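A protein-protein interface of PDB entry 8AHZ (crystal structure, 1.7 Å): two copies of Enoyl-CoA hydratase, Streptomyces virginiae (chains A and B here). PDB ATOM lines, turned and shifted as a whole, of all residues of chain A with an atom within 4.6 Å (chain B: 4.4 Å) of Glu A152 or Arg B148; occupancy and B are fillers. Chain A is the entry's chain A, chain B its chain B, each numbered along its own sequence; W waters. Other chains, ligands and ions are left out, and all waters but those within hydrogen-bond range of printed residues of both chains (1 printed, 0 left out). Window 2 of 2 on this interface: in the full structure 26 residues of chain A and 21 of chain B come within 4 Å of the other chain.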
ATOM      1  N   ALA A 147       6.892  18.961 -10.703  1.00  0.00           N
ATOM      2  CA  ALA A 147       6.477  17.639 -11.229  1.00  0.00           C
ATOM      3  C   ALA A 147       5.073  17.269 -10.708  1.00  0.00           C
ATOM      4  O   ALA A 147       4.391  16.529 -11.371  1.00  0.00           O
ATOM      5  CB  ALA A 147       7.496  16.596 -10.839  1.00  0.00           C
ATOM      6  N   THR A 150       3.198  19.101 -13.647  1.00  0.00           N
ATOM      7  CA  THR A 150       3.494  18.787 -15.061  1.00  0.00           C
ATOM      8  C   THR A 150       3.626  17.283 -15.289  1.00  0.00           C
ATOM      9  O   THR A 150       3.619  16.858 -16.452  1.00  0.00           O
ATOM     10  CB  THR A 150       4.789  19.467 -15.529  1.00  0.00           C
ATOM     11  OG1 THR A 150       5.851  18.894 -14.768  1.00  0.00           O
ATOM     12  CG2 THR A 150       4.781  20.958 -15.343  1.00  0.00           C
ATOM     13  N   GLY A 151       3.813  16.523 -14.221  1.00  0.00           N
ATOM     14  CA  GLY A 151       4.229  15.116 -14.331  1.00  0.00           C
ATOM     15  C   GLY A 151       5.736  15.005 -14.419  1.00  0.00           C
ATOM     16  O   GLY A 151       6.442  15.994 -14.759  1.00  0.00           O
ATOM     17  N   GLU A 152       6.263  13.845 -14.089  1.00  0.00           N
ATOM     18  CA  GLU A 152       7.735  13.656 -13.984  1.00  0.00           C
ATOM     19  C   GLU A 152       8.396  13.928 -15.337  1.00  0.00           C
ATOM     20  O   GLU A 152       9.466  14.543 -15.342  1.00  0.00           O
ATOM     21  CB  GLU A 152       8.063  12.270 -13.409  1.00  0.00           C
ATOM     22  CG  GLU A 152       7.505  11.082 -14.150  1.00  0.00           C
ATOM     23  CD  GLU A 152       8.107   9.746 -13.716  1.00  0.00           C
ATOM     24  OE1 GLU A 152       7.328   8.960 -13.164  1.00  0.00           O
ATOM     25  OE2 GLU A 152       9.344   9.491 -13.970  1.00  0.00           O
ATOM     26  N   GLN A 153       7.888  13.419 -16.454  1.00  0.00           N
ATOM     27  CA  GLN A 153       8.666  13.498 -17.716  1.00  0.00           C
ATOM     28  C   GLN A 153       8.851  14.959 -18.124  1.00  0.00           C
ATOM     29  O   GLN A 153       9.995  15.374 -18.466  1.00  0.00           O
ATOM     30  CB  GLN A 153       7.983  12.714 -18.828  1.00  0.00           C
ATOM     31  CG  GLN A 153       8.670  12.842 -20.164  1.00  0.00           C
ATOM     32  CD  GLN A 153      10.080  12.312 -20.156  1.00  0.00           C
ATOM     33  OE1 GLN A 153      10.427  11.391 -19.405  1.00  0.00           O
ATOM     34  NE2 GLN A 153      10.889  12.845 -21.047  1.00  0.00           N
ATOM     35  N   ARG A 154       7.775  15.745 -18.170  1.00  0.00           N
ATOM     36  CA  ARG A 154       7.929  17.145 -18.668  1.00  0.00           C
ATOM     37  C   ARG A 154       8.780  17.949 -17.665  1.00  0.00           C
ATOM     38  O   ARG A 154       9.578  18.800 -18.135  1.00  0.00           O
ATOM     39  CB  ARG A 154       6.590  17.840 -18.951  1.00  0.00           C
ATOM     40  CG  ARG A 154       6.718  19.158 -19.714  1.00  0.00           C
ATOM     41  CD  ARG A 154       7.633  19.084 -20.925  1.00  0.00           C
ATOM     42  NE  ARG A 154       7.460  20.145 -21.914  1.00  0.00           N
ATOM     43  CZ  ARG A 154       6.448  20.251 -22.759  1.00  0.00           C
ATOM     44  NH1 ARG A 154       5.480  19.349 -22.780  1.00  0.00           N
ATOM     45  NH2 ARG A 154       6.406  21.267 -23.607  1.00  0.00           N
ATOM     46  N   ALA A 155       8.652  17.722 -16.353  1.00  0.00           N
ATOM     47  CA  ALA A 155       9.481  18.449 -15.345  1.00  0.00           C
ATOM     48  C   ALA A 155      10.972  18.145 -15.564  1.00  0.00           C
ATOM     49  O   ALA A 155      11.775  19.087 -15.643  1.00  0.00           O
ATOM     50  CB  ALA A 155       9.069  18.104 -13.935  1.00  0.00           C
ATOM     51  N   PHE A 156      11.331  16.874 -15.724  1.00  0.00           N
ATOM     52  CA  PHE A 156      12.752  16.468 -15.848  1.00  0.00           C
ATOM     53  C   PHE A 156      13.282  16.804 -17.247  1.00  0.00           C
ATOM     54  O   PHE A 156      14.438  17.265 -17.348  1.00  0.00           O
ATOM     55  CB  PHE A 156      12.898  15.010 -15.423  1.00  0.00           C
ATOM     56  CG  PHE A 156      13.012  14.894 -13.925  1.00  0.00           C
ATOM     57  CD1 PHE A 156      11.879  14.844 -13.123  1.00  0.00           C
ATOM     58  CD2 PHE A 156      14.256  14.921 -13.300  1.00  0.00           C
ATOM     59  CE1 PHE A 156      11.985  14.799 -11.738  1.00  0.00           C
ATOM     60  CE2 PHE A 156      14.363  14.893 -11.913  1.00  0.00           C
ATOM     61  CZ  PHE A 156      13.226  14.816 -11.138  1.00  0.00           C
ATOM     62  N   THR B  92      17.318   4.848 -18.491  1.00  0.00           N
ATOM     63  CA  THR B  92      16.782   5.859 -17.558  1.00  0.00           C
ATOM     64  C   THR B  92      17.811   6.242 -16.489  1.00  0.00           C
ATOM     65  O   THR B  92      17.594   7.308 -15.878  1.00  0.00           O
ATOM     66  CB  THR B  92      15.496   5.410 -16.862  1.00  0.00           C
ATOM     67  OG1 THR B  92      15.806   4.439 -15.853  1.00  0.00           O
ATOM     68  CG2 THR B  92      14.464   4.881 -17.821  1.00  0.00           C
ATOM     69  N   ALA B 115      10.810   4.773 -25.323  1.00  0.00           N
ATOM     70  CA  ALA B 115      10.219   5.465 -24.165  1.00  0.00           C
ATOM     71  C   ALA B 115      11.221   5.576 -23.013  1.00  0.00           C
ATOM     72  O   ALA B 115      11.085   6.523 -22.219  1.00  0.00           O
ATOM     73  CB  ALA B 115       8.960   4.780 -23.716  1.00  0.00           C
ATOM     74  N   ALA B 116      12.128   4.604 -22.859  1.00  0.00           N
ATOM     75  CA  ALA B 116      13.097   4.562 -21.745  1.00  0.00           C
ATOM     76  C   ALA B 116      14.180   5.614 -21.961  1.00  0.00           C
ATOM     77  O   ALA B 116      14.927   5.901 -21.013  1.00  0.00           O
ATOM     78  CB  ALA B 116      13.672   3.177 -21.641  1.00  0.00           C
ATOM     79  N   CYS B 117      14.297   6.193 -23.159  1.00  0.00           N
ATOM     80  CA  CYS B 117      15.287   7.270 -23.383  1.00  0.00           C
ATOM     81  C   CYS B 117      14.825   8.550 -22.684  1.00  0.00           C
ATOM     82  O   CYS B 117      13.602   8.788 -22.517  1.00  0.00           O
ATOM     83  CB  CYS B 117      15.585   7.502 -24.859  1.00  0.00           C
ATOM     84  SG  CYS B 117      16.409   6.075 -25.637  1.00  0.00           S
ATOM     85  N   PRO B 144       6.038   0.560 -17.479  1.00  0.00           N
ATOM     86  CA  PRO B 144       6.496   1.621 -16.585  1.00  0.00           C
ATOM     87  C   PRO B 144       7.193   2.741 -17.341  1.00  0.00           C
ATOM     88  O   PRO B 144       7.080   3.901 -16.955  1.00  0.00           O
ATOM     89  CB  PRO B 144       7.467   0.893 -15.634  1.00  0.00           C
ATOM     90  CG  PRO B 144       6.975  -0.517 -15.654  1.00  0.00           C
ATOM     91  CD  PRO B 144       6.552  -0.758 -17.096  1.00  0.00           C
ATOM     92  N   PHE B 145       7.888   2.404 -18.421  1.00  0.00           N
ATOM     93  CA  PHE B 145       8.658   3.413 -19.190  1.00  0.00           C
ATOM     94  C   PHE B 145       7.717   4.264 -20.052  1.00  0.00           C
ATOM     95  O   PHE B 145       8.055   5.393 -20.359  1.00  0.00           O
ATOM     96  CB  PHE B 145       9.789   2.703 -19.929  1.00  0.00           C
ATOM     97  CG  PHE B 145      10.652   1.928 -18.971  1.00  0.00           C
ATOM     98  CD1 PHE B 145      11.654   2.561 -18.258  1.00  0.00           C
ATOM     99  CD2 PHE B 145      10.408   0.589 -18.715  1.00  0.00           C
ATOM    100  CE1 PHE B 145      12.424   1.860 -17.346  1.00  0.00           C
ATOM    101  CE2 PHE B 145      11.179  -0.109 -17.803  1.00  0.00           C
ATOM    102  CZ  PHE B 145      12.183   0.528 -17.119  1.00  0.00           C
ATOM    103  N   VAL B 146       6.582   3.690 -20.439  1.00  0.00           N
ATOM    104  CA  VAL B 146       5.570   4.482 -21.187  1.00  0.00           C
ATOM    105  C   VAL B 146       4.771   5.325 -20.184  1.00  0.00           C
ATOM    106  O   VAL B 146       4.568   6.491 -20.462  1.00  0.00           O
ATOM    107  CB  VAL B 146       4.638   3.557 -21.993  1.00  0.00           C
ATOM    108  CG1 VAL B 146       3.521   4.321 -22.681  1.00  0.00           C
ATOM    109  CG2 VAL B 146       5.410   2.713 -22.993  1.00  0.00           C
ATOM    110  N   ALA B 147       4.386   4.731 -19.052  1.00  0.00           N
ATOM    111  CA  ALA B 147       3.512   5.408 -18.074  1.00  0.00           C
ATOM    112  C   ALA B 147       4.273   6.558 -17.403  1.00  0.00           C
ATOM    113  O   ALA B 147       3.636   7.552 -17.053  1.00  0.00           O
ATOM    114  CB  ALA B 147       2.992   4.421 -17.063  1.00  0.00           C
ATOM    115  N   ARG B 148       5.597   6.480 -17.303  1.00  0.00           N
ATOM    116  CA  ARG B 148       6.356   7.610 -16.706  1.00  0.00           C
ATOM    117  C   ARG B 148       6.358   8.796 -17.671  1.00  0.00           C
ATOM    118  O   ARG B 148       6.670   9.916 -17.221  1.00  0.00           O
ATOM    119  CB  ARG B 148       7.787   7.205 -16.390  1.00  0.00           C
ATOM    120  CG  ARG B 148       8.644   7.109 -17.632  1.00  0.00           C
ATOM    121  CD  ARG B 148      10.036   6.607 -17.344  1.00  0.00           C
ATOM    122  NE  ARG B 148      10.745   6.846 -18.599  1.00  0.00           N
ATOM    123  CZ  ARG B 148      11.887   7.543 -18.703  1.00  0.00           C
ATOM    124  NH1 ARG B 148      12.527   7.933 -17.628  1.00  0.00           N
ATOM    125  NH2 ARG B 148      12.421   7.734 -19.899  1.00  0.00           N
ATOM    126  N   ARG B 149       5.993   8.580 -18.942  1.00  0.00           N
ATOM    127  CA  ARG B 149       5.855   9.675 -19.936  1.00  0.00           C
ATOM    128  C   ARG B 149       4.408  10.124 -20.111  1.00  0.00           C
ATOM    129  O   ARG B 149       4.194  11.342 -20.227  1.00  0.00           O
ATOM    130  CB  ARG B 149       6.398   9.225 -21.296  1.00  0.00           C
ATOM    131  CG  ARG B 149       7.911   9.094 -21.344  1.00  0.00           C
ATOM    132  CD  ARG B 149       8.377   8.585 -22.699  1.00  0.00           C
ATOM    133  NE  ARG B 149       9.771   8.954 -22.889  1.00  0.00           N
ATOM    134  CZ  ARG B 149      10.189  10.161 -23.221  1.00  0.00           C
ATOM    135  NH1 ARG B 149       9.333  11.122 -23.512  1.00  0.00           N
ATOM    136  NH2 ARG B 149      11.480  10.427 -23.245  1.00  0.00           N
ATOM    137  N   THR B 150       3.471   9.184 -20.223  1.00  0.00           N
ATOM    138  CA  THR B 150       2.078   9.474 -20.654  1.00  0.00           C
ATOM    139  C   THR B 150       1.159   9.642 -19.452  1.00  0.00           C
ATOM    140  O   THR B 150       0.015  10.115 -19.648  1.00  0.00           O
ATOM    141  CB  THR B 150       1.529   8.383 -21.581  1.00  0.00           C
ATOM    142  OG1 THR B 150       1.436   7.175 -20.829  1.00  0.00           O
ATOM    143  CG2 THR B 150       2.403   8.136 -22.795  1.00  0.00           C
ATOM    144  N   ARG B 209      15.784  11.990 -10.375  1.00  0.00           N
ATOM    145  CA  ARG B 209      14.484  11.521 -10.912  1.00  0.00           C
ATOM    146  C   ARG B 209      14.145  10.168 -10.286  1.00  0.00           C
ATOM    147  O   ARG B 209      12.987   9.949  -9.910  1.00  0.00           O
ATOM    148  CB  ARG B 209      14.488  11.405 -12.437  1.00  0.00           C
ATOM    149  CG  ARG B 209      13.104  11.122 -13.001  1.00  0.00           C
ATOM    150  CD  ARG B 209      13.107  11.113 -14.510  1.00  0.00           C
ATOM    151  NE  ARG B 209      11.811  10.737 -15.050  1.00  0.00           N
ATOM    152  CZ  ARG B 209      11.451  10.889 -16.317  1.00  0.00           C
ATOM    153  NH1 ARG B 209      12.283  11.448 -17.185  1.00  0.00           N
ATOM    154  NH2 ARG B 209      10.246  10.508 -16.697  1.00  0.00           N
ATOM    155  N   PHE B 213      10.801   9.638  -8.155  1.00  0.00           N
ATOM    156  CA  PHE B 213       9.854   8.759  -8.888  1.00  0.00           C
ATOM    157  C   PHE B 213      10.472   7.378  -9.026  1.00  0.00           C
ATOM    158  O   PHE B 213      10.820   6.957 -10.121  1.00  0.00           O
ATOM    159  CB  PHE B 213       9.515   9.365 -10.256  1.00  0.00           C
ATOM    160  CG  PHE B 213       8.709  10.627 -10.131  1.00  0.00           C
ATOM    161  CD1 PHE B 213       7.332  10.555 -10.007  1.00  0.00           C
ATOM    162  CD2 PHE B 213       9.317  11.873 -10.169  1.00  0.00           C
ATOM    163  CE1 PHE B 213       6.566  11.699  -9.859  1.00  0.00           C
ATOM    164  CE2 PHE B 213       8.552  13.021 -10.022  1.00  0.00           C
ATOM    165  CZ  PHE B 213       7.186  12.929  -9.888  1.00  0.00           C
HETATM  166  O   HOH W   1      10.386   7.228 -13.160  1.00  0.00           O
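Of the 8 printed residues of chain A, 4 touch a printed residue of chain B. Of the 13 printed residues of chain B, 4 touch a printed residue of chain A. Hydrophobic or aromatic side chains of chain B that line the printed part of chain A: Phe B213. Among the printed residues, 8 pairs touch across the chains. Among the printed residues, Asp or Glu carboxylates within 4 Å of a Lys or Arg side-chain nitrogen of the other chain: Glu A152 with Arg B209 (3.0 Å).
Glu A152 touches three residues of chain B. Of the printed residues of chain A, Arg B209 touches Glu A152 (3.0 Å), Gln A153 (2.9 Å) and Phe A156 (3.5 Å). Printed residues of chain B within 4 Å of Ala A147: Phe B213. Of the printed residues of chain B, Phe A156 touches Arg B209. Of the printed residues of chain A, Phe B213 touches Ala A147 (3.8 Å) and Glu A152 (3.5 Å). Val B146 touches none of the printed residues of chain A. Phe B145 touches none of the printed residues of chain A. The nearest printed residue of chain A that does not touch Phe B213 is Phe A156 (4.2 Å).
O of Ala B116 is in hydrogen-bond range of NH2 of Arg B148. The guanidinium group (NH2) of Arg B149 is in hydrogen-bond range of the backbone carbonyl oxygen (O) of Cys B117 (2.8 Å). O of Ala B115 is in hydrogen-bond range of NH2 of Arg B148, 2.9 Å away. The backbone carbonyl oxygen (O) of Ala B115 is in hydrogen-bond range of the guanidinium group (NE) of Arg B149 (2.8 Å). The backbone carbonyl oxygen (O) of Cys B117 lies within hydrogen-bond range of the guanidinium group (NH2) of Arg B148 (3.1 Å).
Among the printed residues, pairs that only touch across the chains: Ala A147 with Phe B213 (3.8 Å), Glu A152 with Arg B148 (3.4 Å), Glu A152 with Phe B213 (3.5 Å), Gln A153 with Arg B148 (3.5 Å) and Phe A156 with Arg B209 (3.5 Å).
Water W1 lies within hydrogen-bond range of OE2 of Glu A152 (2.6 Å) and O of Phe B213 (3.1 Å).
Positions printed for both chains: 147 and 150. Of the 8 pairs that touch across the chains among the printed residues, none has its exchanged pair printed and touching as well.
The side-chain amide nitrogen (NE2) of Gln A153 lies close to the guanidinium group (NH2) of Arg B149 (3.3 Å). OE2 of Glu A152 is in salt-bridge range of NE of Arg B209 (3.0 Å). OE1 of Gln A153 sits at hydrogen-bond distance from NH2 of Arg B209 (2.9 Å).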
